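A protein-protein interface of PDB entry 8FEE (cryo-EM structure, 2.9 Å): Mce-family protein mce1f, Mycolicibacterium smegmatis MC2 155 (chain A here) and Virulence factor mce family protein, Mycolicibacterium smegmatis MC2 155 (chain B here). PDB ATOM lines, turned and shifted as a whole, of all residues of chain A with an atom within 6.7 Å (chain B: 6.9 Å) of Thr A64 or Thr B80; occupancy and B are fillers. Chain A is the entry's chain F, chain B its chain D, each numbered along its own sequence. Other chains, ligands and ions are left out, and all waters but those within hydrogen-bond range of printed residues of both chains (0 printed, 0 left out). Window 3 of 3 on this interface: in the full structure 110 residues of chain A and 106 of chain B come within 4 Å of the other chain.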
ATOM      1  N   VAL A  59      25.725   8.409  -3.453  1.00  0.00           N
ATOM      2  CA  VAL A  59      24.893   8.026  -4.586  1.00  0.00           C
ATOM      3  C   VAL A  59      23.940   9.177  -4.854  1.00  0.00           C
ATOM      4  O   VAL A  59      23.240   9.631  -3.941  1.00  0.00           O
ATOM      5  CB  VAL A  59      24.123   6.726  -4.304  1.00  0.00           C
ATOM      6  CG1 VAL A  59      23.109   6.460  -5.400  1.00  0.00           C
ATOM      7  CG2 VAL A  59      25.084   5.564  -4.165  1.00  0.00           C
ATOM      8  N   THR A  60      23.922   9.668  -6.088  1.00  0.00           N
ATOM      9  CA  THR A  60      23.149  10.851  -6.430  1.00  0.00           C
ATOM     10  C   THR A  60      22.169  10.547  -7.552  1.00  0.00           C
ATOM     11  O   THR A  60      22.383   9.645  -8.366  1.00  0.00           O
ATOM     12  CB  THR A  60      24.057  12.013  -6.849  1.00  0.00           C
ATOM     13  OG1 THR A  60      24.751  11.668  -8.053  1.00  0.00           O
ATOM     14  CG2 THR A  60      25.067  12.328  -5.757  1.00  0.00           C
ATOM     15  N   TYR A  61      21.082  11.307  -7.571  1.00  0.00           N
ATOM     16  CA  TYR A  61      20.103  11.298  -8.655  1.00  0.00           C
ATOM     17  C   TYR A  61      20.075  12.715  -9.217  1.00  0.00           C
ATOM     18  O   TYR A  61      19.416  13.593  -8.652  1.00  0.00           O
ATOM     19  CB  TYR A  61      18.731  10.845  -8.162  1.00  0.00           C
ATOM     20  CG  TYR A  61      17.672  10.757  -9.241  1.00  0.00           C
ATOM     21  CD1 TYR A  61      16.950  11.877  -9.634  1.00  0.00           C
ATOM     22  CD2 TYR A  61      17.390   9.549  -9.863  1.00  0.00           C
ATOM     23  CE1 TYR A  61      15.985  11.796 -10.619  1.00  0.00           C
ATOM     24  CE2 TYR A  61      16.425   9.459 -10.848  1.00  0.00           C
ATOM     25  CZ  TYR A  61      15.725  10.585 -11.221  1.00  0.00           C
ATOM     26  OH  TYR A  61      14.763  10.505 -12.201  1.00  0.00           O
ATOM     27  N   ARG A  62      20.796  12.931 -10.321  1.00  0.00           N
ATOM     28  CA  ARG A  62      20.961  14.255 -10.928  1.00  0.00           C
ATOM     29  C   ARG A  62      21.611  15.237  -9.954  1.00  0.00           C
ATOM     30  O   ARG A  62      21.263  16.418  -9.907  1.00  0.00           O
ATOM     31  CB  ARG A  62      19.632  14.807 -11.454  1.00  0.00           C
ATOM     32  CG  ARG A  62      19.049  14.028 -12.617  1.00  0.00           C
ATOM     33  CD  ARG A  62      17.733  14.633 -13.071  1.00  0.00           C
ATOM     34  NE  ARG A  62      17.235  14.004 -14.288  1.00  0.00           N
ATOM     35  CZ  ARG A  62      17.540  14.402 -15.515  1.00  0.00           C
ATOM     36  NH1 ARG A  62      18.348  15.428 -15.726  1.00  0.00           N
ATOM     37  NH2 ARG A  62      17.023  13.755 -16.554  1.00  0.00           N
ATOM     38  N   GLY A  63      22.564  14.740  -9.166  1.00  0.00           N
ATOM     39  CA  GLY A  63      23.388  15.563  -8.311  1.00  0.00           C
ATOM     40  C   GLY A  63      22.963  15.624  -6.857  1.00  0.00           C
ATOM     41  O   GLY A  63      23.781  15.994  -6.007  1.00  0.00           O
ATOM     42  N   THR A  64      21.718  15.276  -6.541  1.00  0.00           N
ATOM     43  CA  THR A  64      21.252  15.306  -5.161  1.00  0.00           C
ATOM     44  C   THR A  64      21.426  13.927  -4.533  1.00  0.00           C
ATOM     45  O   THR A  64      21.156  12.902  -5.163  1.00  0.00           O
ATOM     46  CB  THR A  64      19.792  15.775  -5.070  1.00  0.00           C
ATOM     47  OG1 THR A  64      19.418  15.912  -3.693  1.00  0.00           O
ATOM     48  CG2 THR A  64      18.837  14.807  -5.753  1.00  0.00           C
ATOM     49  N   THR A  65      21.928  13.907  -3.300  1.00  0.00           N
ATOM     50  CA  THR A  65      22.289  12.652  -2.659  1.00  0.00           C
ATOM     51  C   THR A  65      21.037  11.920  -2.191  1.00  0.00           C
ATOM     52  O   THR A  65      20.172  12.506  -1.533  1.00  0.00           O
ATOM     53  CB  THR A  65      23.226  12.911  -1.478  1.00  0.00           C
ATOM     54  OG1 THR A  65      24.454  13.476  -1.956  1.00  0.00           O
ATOM     55  CG2 THR A  65      23.528  11.620  -0.737  1.00  0.00           C
ATOM     56  N   ILE A  66      20.944  10.636  -2.538  1.00  0.00           N
ATOM     57  CA  ILE A  66      19.826   9.788  -2.141  1.00  0.00           C
ATOM     58  C   ILE A  66      20.354   8.479  -1.569  1.00  0.00           C
ATOM     59  O   ILE A  66      19.603   7.510  -1.415  1.00  0.00           O
ATOM     60  CB  ILE A  66      18.873   9.519  -3.323  1.00  0.00           C
ATOM     61  CG1 ILE A  66      19.561   8.649  -4.379  1.00  0.00           C
ATOM     62  CG2 ILE A  66      18.373  10.819  -3.935  1.00  0.00           C
ATOM     63  CD1 ILE A  66      18.621   8.113  -5.431  1.00  0.00           C
ATOM     64  N   GLY A  67      21.643   8.433  -1.253  1.00  0.00           N
ATOM     65  CA  GLY A  67      22.213   7.220  -0.707  1.00  0.00           C
ATOM     66  C   GLY A  67      23.721   7.320  -0.586  1.00  0.00           C
ATOM     67  O   GLY A  67      24.312   8.382  -0.791  1.00  0.00           O
ATOM     68  N   TYR A  89      13.046   7.332  -1.909  1.00  0.00           N
ATOM     69  CA  TYR A  89      13.396   7.624  -3.292  1.00  0.00           C
ATOM     70  C   TYR A  89      13.205   6.371  -4.138  1.00  0.00           C
ATOM     71  O   TYR A  89      13.837   5.341  -3.880  1.00  0.00           O
ATOM     72  CB  TYR A  89      14.835   8.126  -3.404  1.00  0.00           C
ATOM     73  CG  TYR A  89      15.065   9.485  -2.788  1.00  0.00           C
ATOM     74  CD1 TYR A  89      14.803  10.645  -3.505  1.00  0.00           C
ATOM     75  CD2 TYR A  89      15.558   9.610  -1.498  1.00  0.00           C
ATOM     76  CE1 TYR A  89      15.014  11.891  -2.948  1.00  0.00           C
ATOM     77  CE2 TYR A  89      15.773  10.853  -0.933  1.00  0.00           C
ATOM     78  CZ  TYR A  89      15.500  11.990  -1.662  1.00  0.00           C
ATOM     79  OH  TYR A  89      15.714  13.228  -1.103  1.00  0.00           O
ATOM     80  N   ASP A 111      26.154   8.684 -10.087  1.00  0.00           N
ATOM     81  CA  ASP A 111      24.895   9.345 -10.389  1.00  0.00           C
ATOM     82  C   ASP A 111      24.003   8.367 -11.137  1.00  0.00           C
ATOM     83  O   ASP A 111      24.450   7.707 -12.080  1.00  0.00           O
ATOM     84  CB  ASP A 111      25.132  10.611 -11.218  1.00  0.00           C
ATOM     85  CG  ASP A 111      23.894  11.494 -11.328  1.00  0.00           C
ATOM     86  OD1 ASP A 111      22.781  10.976 -11.559  1.00  0.00           O
ATOM     87  OD2 ASP A 111      24.039  12.725 -11.181  1.00  0.00           O
ATOM     88  N   VAL B  56      21.378  19.506 -10.787  1.00  0.00           N
ATOM     89  CA  VAL B  56      21.758  20.303  -9.620  1.00  0.00           C
ATOM     90  C   VAL B  56      22.866  19.527  -8.914  1.00  0.00           C
ATOM     91  O   VAL B  56      22.602  18.642  -8.094  1.00  0.00           O
ATOM     92  CB  VAL B  56      20.578  20.582  -8.684  1.00  0.00           C
ATOM     93  CG1 VAL B  56      21.046  21.266  -7.419  1.00  0.00           C
ATOM     94  CG2 VAL B  56      19.554  21.457  -9.380  1.00  0.00           C
ATOM     95  N   LEU B  57      24.114  19.841  -9.242  1.00  0.00           N
ATOM     96  CA  LEU B  57      25.274  19.140  -8.709  1.00  0.00           C
ATOM     97  C   LEU B  57      26.049  20.068  -7.784  1.00  0.00           C
ATOM     98  O   LEU B  57      26.308  21.222  -8.137  1.00  0.00           O
ATOM     99  CB  LEU B  57      26.181  18.638  -9.835  1.00  0.00           C
ATOM    100  CG  LEU B  57      27.535  18.085  -9.388  1.00  0.00           C
ATOM    101  CD1 LEU B  57      27.341  16.877  -8.490  1.00  0.00           C
ATOM    102  CD2 LEU B  57      28.396  17.724 -10.584  1.00  0.00           C
ATOM    103  N   ALA B  58      26.398  19.560  -6.601  1.00  0.00           N
ATOM    104  CA  ALA B  58      27.171  20.275  -5.585  1.00  0.00           C
ATOM    105  C   ALA B  58      26.481  21.551  -5.118  1.00  0.00           C
ATOM    106  O   ALA B  58      27.130  22.451  -4.574  1.00  0.00           O
ATOM    107  CB  ALA B  58      28.590  20.587  -6.073  1.00  0.00           C
ATOM    108  N   LEU B  59      25.171  21.646  -5.316  1.00  0.00           N
ATOM    109  CA  LEU B  59      24.361  22.732  -4.786  1.00  0.00           C
ATOM    110  C   LEU B  59      23.487  22.172  -3.675  1.00  0.00           C
ATOM    111  O   LEU B  59      22.794  21.168  -3.872  1.00  0.00           O
ATOM    112  CB  LEU B  59      23.502  23.366  -5.881  1.00  0.00           C
ATOM    113  CG  LEU B  59      22.730  24.625  -5.495  1.00  0.00           C
ATOM    114  CD1 LEU B  59      23.648  25.827  -5.545  1.00  0.00           C
ATOM    115  CD2 LEU B  59      21.532  24.821  -6.406  1.00  0.00           C
ATOM    116  N   TYR B  60      23.529  22.808  -2.515  1.00  0.00           N
ATOM    117  CA  TYR B  60      22.881  22.314  -1.313  1.00  0.00           C
ATOM    118  C   TYR B  60      21.997  23.402  -0.730  1.00  0.00           C
ATOM    119  O   TYR B  60      22.208  24.590  -0.995  1.00  0.00           O
ATOM    120  CB  TYR B  60      23.930  21.877  -0.279  1.00  0.00           C
ATOM    121  CG  TYR B  60      25.050  21.065  -0.882  1.00  0.00           C
ATOM    122  CD1 TYR B  60      24.807  19.817  -1.437  1.00  0.00           C
ATOM    123  CD2 TYR B  60      26.348  21.552  -0.910  1.00  0.00           C
ATOM    124  CE1 TYR B  60      25.826  19.075  -1.997  1.00  0.00           C
ATOM    125  CE2 TYR B  60      27.373  20.816  -1.465  1.00  0.00           C
ATOM    126  CZ  TYR B  60      27.108  19.580  -2.008  1.00  0.00           C
ATOM    127  OH  TYR B  60      28.127  18.845  -2.564  1.00  0.00           O
ATOM    128  N   ILE B  78      15.854  21.707  -2.148  1.00  0.00           N
ATOM    129  CA  ILE B  78      16.126  21.091  -3.445  1.00  0.00           C
ATOM    130  C   ILE B  78      15.476  19.714  -3.447  1.00  0.00           C
ATOM    131  O   ILE B  78      15.843  18.857  -2.635  1.00  0.00           O
ATOM    132  CB  ILE B  78      17.633  20.964  -3.729  1.00  0.00           C
ATOM    133  CG1 ILE B  78      18.284  22.343  -3.822  1.00  0.00           C
ATOM    134  CG2 ILE B  78      17.871  20.168  -5.000  1.00  0.00           C
ATOM    135  CD1 ILE B  78      19.776  22.294  -4.002  1.00  0.00           C
ATOM    136  N   GLU B  79      14.518  19.490  -4.347  1.00  0.00           N
ATOM    137  CA  GLU B  79      13.886  18.180  -4.441  1.00  0.00           C
ATOM    138  C   GLU B  79      13.629  17.813  -5.895  1.00  0.00           C
ATOM    139  O   GLU B  79      13.390  18.676  -6.739  1.00  0.00           O
ATOM    140  CB  GLU B  79      12.571  18.122  -3.645  1.00  0.00           C
ATOM    141  CG  GLU B  79      11.459  19.024  -4.161  1.00  0.00           C
ATOM    142  CD  GLU B  79      11.579  20.456  -3.675  1.00  0.00           C
ATOM    143  OE1 GLU B  79      12.591  20.791  -3.024  1.00  0.00           O
ATOM    144  OE2 GLU B  79      10.655  21.250  -3.944  1.00  0.00           O
ATOM    145  N   THR B  80      13.686  16.514  -6.177  1.00  0.00           N
ATOM    146  CA  THR B  80      13.489  16.027  -7.535  1.00  0.00           C
ATOM    147  C   THR B  80      12.027  16.158  -7.947  1.00  0.00           C
ATOM    148  O   THR B  80      11.117  15.855  -7.170  1.00  0.00           O
ATOM    149  CB  THR B  80      13.935  14.568  -7.636  1.00  0.00           C
ATOM    150  OG1 THR B  80      15.315  14.461  -7.270  1.00  0.00           O
ATOM    151  CG2 THR B  80      13.755  14.042  -9.050  1.00  0.00           C
ATOM    152  N   ALA B  81      11.799  16.614  -9.179  1.00  0.00           N
ATOM    153  CA  ALA B  81      10.463  16.727  -9.756  1.00  0.00           C
ATOM    154  C   ALA B  81      10.532  16.139 -11.163  1.00  0.00           C
ATOM    155  O   ALA B  81      10.937  16.824 -12.107  1.00  0.00           O
ATOM    156  CB  ALA B  81       9.983  18.174  -9.775  1.00  0.00           C
ATOM    157  N   GLY B  82      10.132  14.876 -11.294  1.00  0.00           N
ATOM    158  CA  GLY B  82      10.188  14.215 -12.589  1.00  0.00           C
ATOM    159  C   GLY B  82      11.616  14.108 -13.082  1.00  0.00           C
ATOM    160  O   GLY B  82      12.508  13.627 -12.374  1.00  0.00           O
ATOM    161  N   ASP B  83      11.845  14.560 -14.312  1.00  0.00           N
ATOM    162  CA  ASP B  83      13.180  14.601 -14.891  1.00  0.00           C
ATOM    163  C   ASP B  83      13.899  15.914 -14.609  1.00  0.00           C
ATOM    164  O   ASP B  83      14.983  16.141 -15.156  1.00  0.00           O
ATOM    165  CB  ASP B  83      13.110  14.361 -16.400  1.00  0.00           C
ATOM    166  CG  ASP B  83      12.288  15.410 -17.119  1.00  0.00           C
ATOM    167  OD1 ASP B  83      11.369  15.979 -16.492  1.00  0.00           O
ATOM    168  OD2 ASP B  83      12.559  15.665 -18.310  1.00  0.00           O
ATOM    169  N   LYS B  84      13.322  16.778 -13.781  1.00  0.00           N
ATOM    170  CA  LYS B  84      13.928  18.047 -13.409  1.00  0.00           C
ATOM    171  C   LYS B  84      14.234  18.062 -11.917  1.00  0.00           C
ATOM    172  O   LYS B  84      13.847  17.166 -11.163  1.00  0.00           O
ATOM    173  CB  LYS B  84      13.008  19.221 -13.770  1.00  0.00           C
ATOM    174  CG  LYS B  84      12.567  19.242 -15.221  1.00  0.00           C
ATOM    175  CD  LYS B  84      11.516  20.312 -15.456  1.00  0.00           C
ATOM    176  CE  LYS B  84      11.024  20.295 -16.894  1.00  0.00           C
ATOM    177  NZ  LYS B  84       9.983  21.332 -17.138  1.00  0.00           N
ATOM    178  N   MET B  85      14.930  19.111 -11.492  1.00  0.00           N
ATOM    179  CA  MET B  85      15.193  19.361 -10.082  1.00  0.00           C
ATOM    180  C   MET B  85      14.597  20.709  -9.711  1.00  0.00           C
ATOM    181  O   MET B  85      14.947  21.730 -10.312  1.00  0.00           O
ATOM    182  CB  MET B  85      16.694  19.339  -9.794  1.00  0.00           C
ATOM    183  CG  MET B  85      17.381  18.039 -10.164  1.00  0.00           C
ATOM    184  SD  MET B  85      16.739  16.660  -9.207  1.00  0.00           S
ATOM    185  CE  MET B  85      16.937  17.310  -7.551  1.00  0.00           C
ATOM    186  N   LYS B  86      13.691  20.707  -8.738  1.00  0.00           N
ATOM    187  CA  LYS B  86      13.004  21.909  -8.293  1.00  0.00           C
ATOM    188  C   LYS B  86      13.758  22.475  -7.097  1.00  0.00           C
ATOM    189  O   LYS B  86      13.905  21.798  -6.070  1.00  0.00           O
ATOM    190  CB  LYS B  86      11.554  21.586  -7.939  1.00  0.00           C
ATOM    191  CG  LYS B  86      10.848  22.614  -7.079  1.00  0.00           C
ATOM    192  CD  LYS B  86       9.391  22.217  -6.884  1.00  0.00           C
ATOM    193  CE  LYS B  86       8.675  23.137  -5.912  1.00  0.00           C
ATOM    194  NZ  LYS B  86       9.167  22.964  -4.520  1.00  0.00           N
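The backbone carbonyl oxygen (O) of Arg A62 is in hydrogen-bond range of the backbone NH (N) of Val B56 (3.2 Å).
The guanidinium group (NE) of Arg A62 lies close to the backbone carbonyl oxygen (O) of Asp B83.
OG1 of Thr B80 is in hydrogen-bond range of SD of Met B85, at 3.3 Å.
N of Arg A62 lies within hydrogen-bond range of OD1 of Asp A111 (3.0 Å).
The side-chain carboxylate of Asp A111 is in hydrogen-bond range of the backbone NH of Gly A63 (3.2 Å).
Tyr A61 touches Thr B80.
Tyr A61 touches Gly B82 (OH to O, 3.9 Å).
CA of Gly A63 touches O of Val B56 (3.2 Å).
N of Thr A64 touches O of Val B56, 3.8 Å away.
Thr A64 touches Thr B80.
Thr A64 touches Met B85.
Of the printed residues of chain B, Arg A62 touches Val B56 (3.2 Å) and Asp B83 (3.1 Å).
Thr A64 touches just these residues of chain B: Val B56 (3.8 Å), Thr B80 (3.9 Å) and Met B85 (3.6 Å).
Leu B59 touches none of the printed residues of chain A.
Glu B79 touches none of the printed residues of chain A.
Of chain A, only Tyr A61 and Thr A64 come within 4 Å of Thr B80.
Printed residues of chain A within 4 Å of Gly B82: Tyr A61.
Printed residues of chain A within 4 Å of Met B85: Thr A64 (3.6 Å).
The nearest residue of chain B that does not touch Thr A64 is Ile B78 (4.7 Å).
The nearest residue of chain A that does not touch Thr B80 is Tyr A89 (5.0 Å).
Hydrophobic or aromatic side chains of chain B that line the printed part of chain A: Met B85.
Hydrophobic or aromatic side chains of chain A within 4 Å of the printed part of chain B: Tyr A61.
Among the printed residues, no Asp or Glu carboxylate lies within 4 Å of a Lys or Arg side-chain nitrogen of the other chain.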
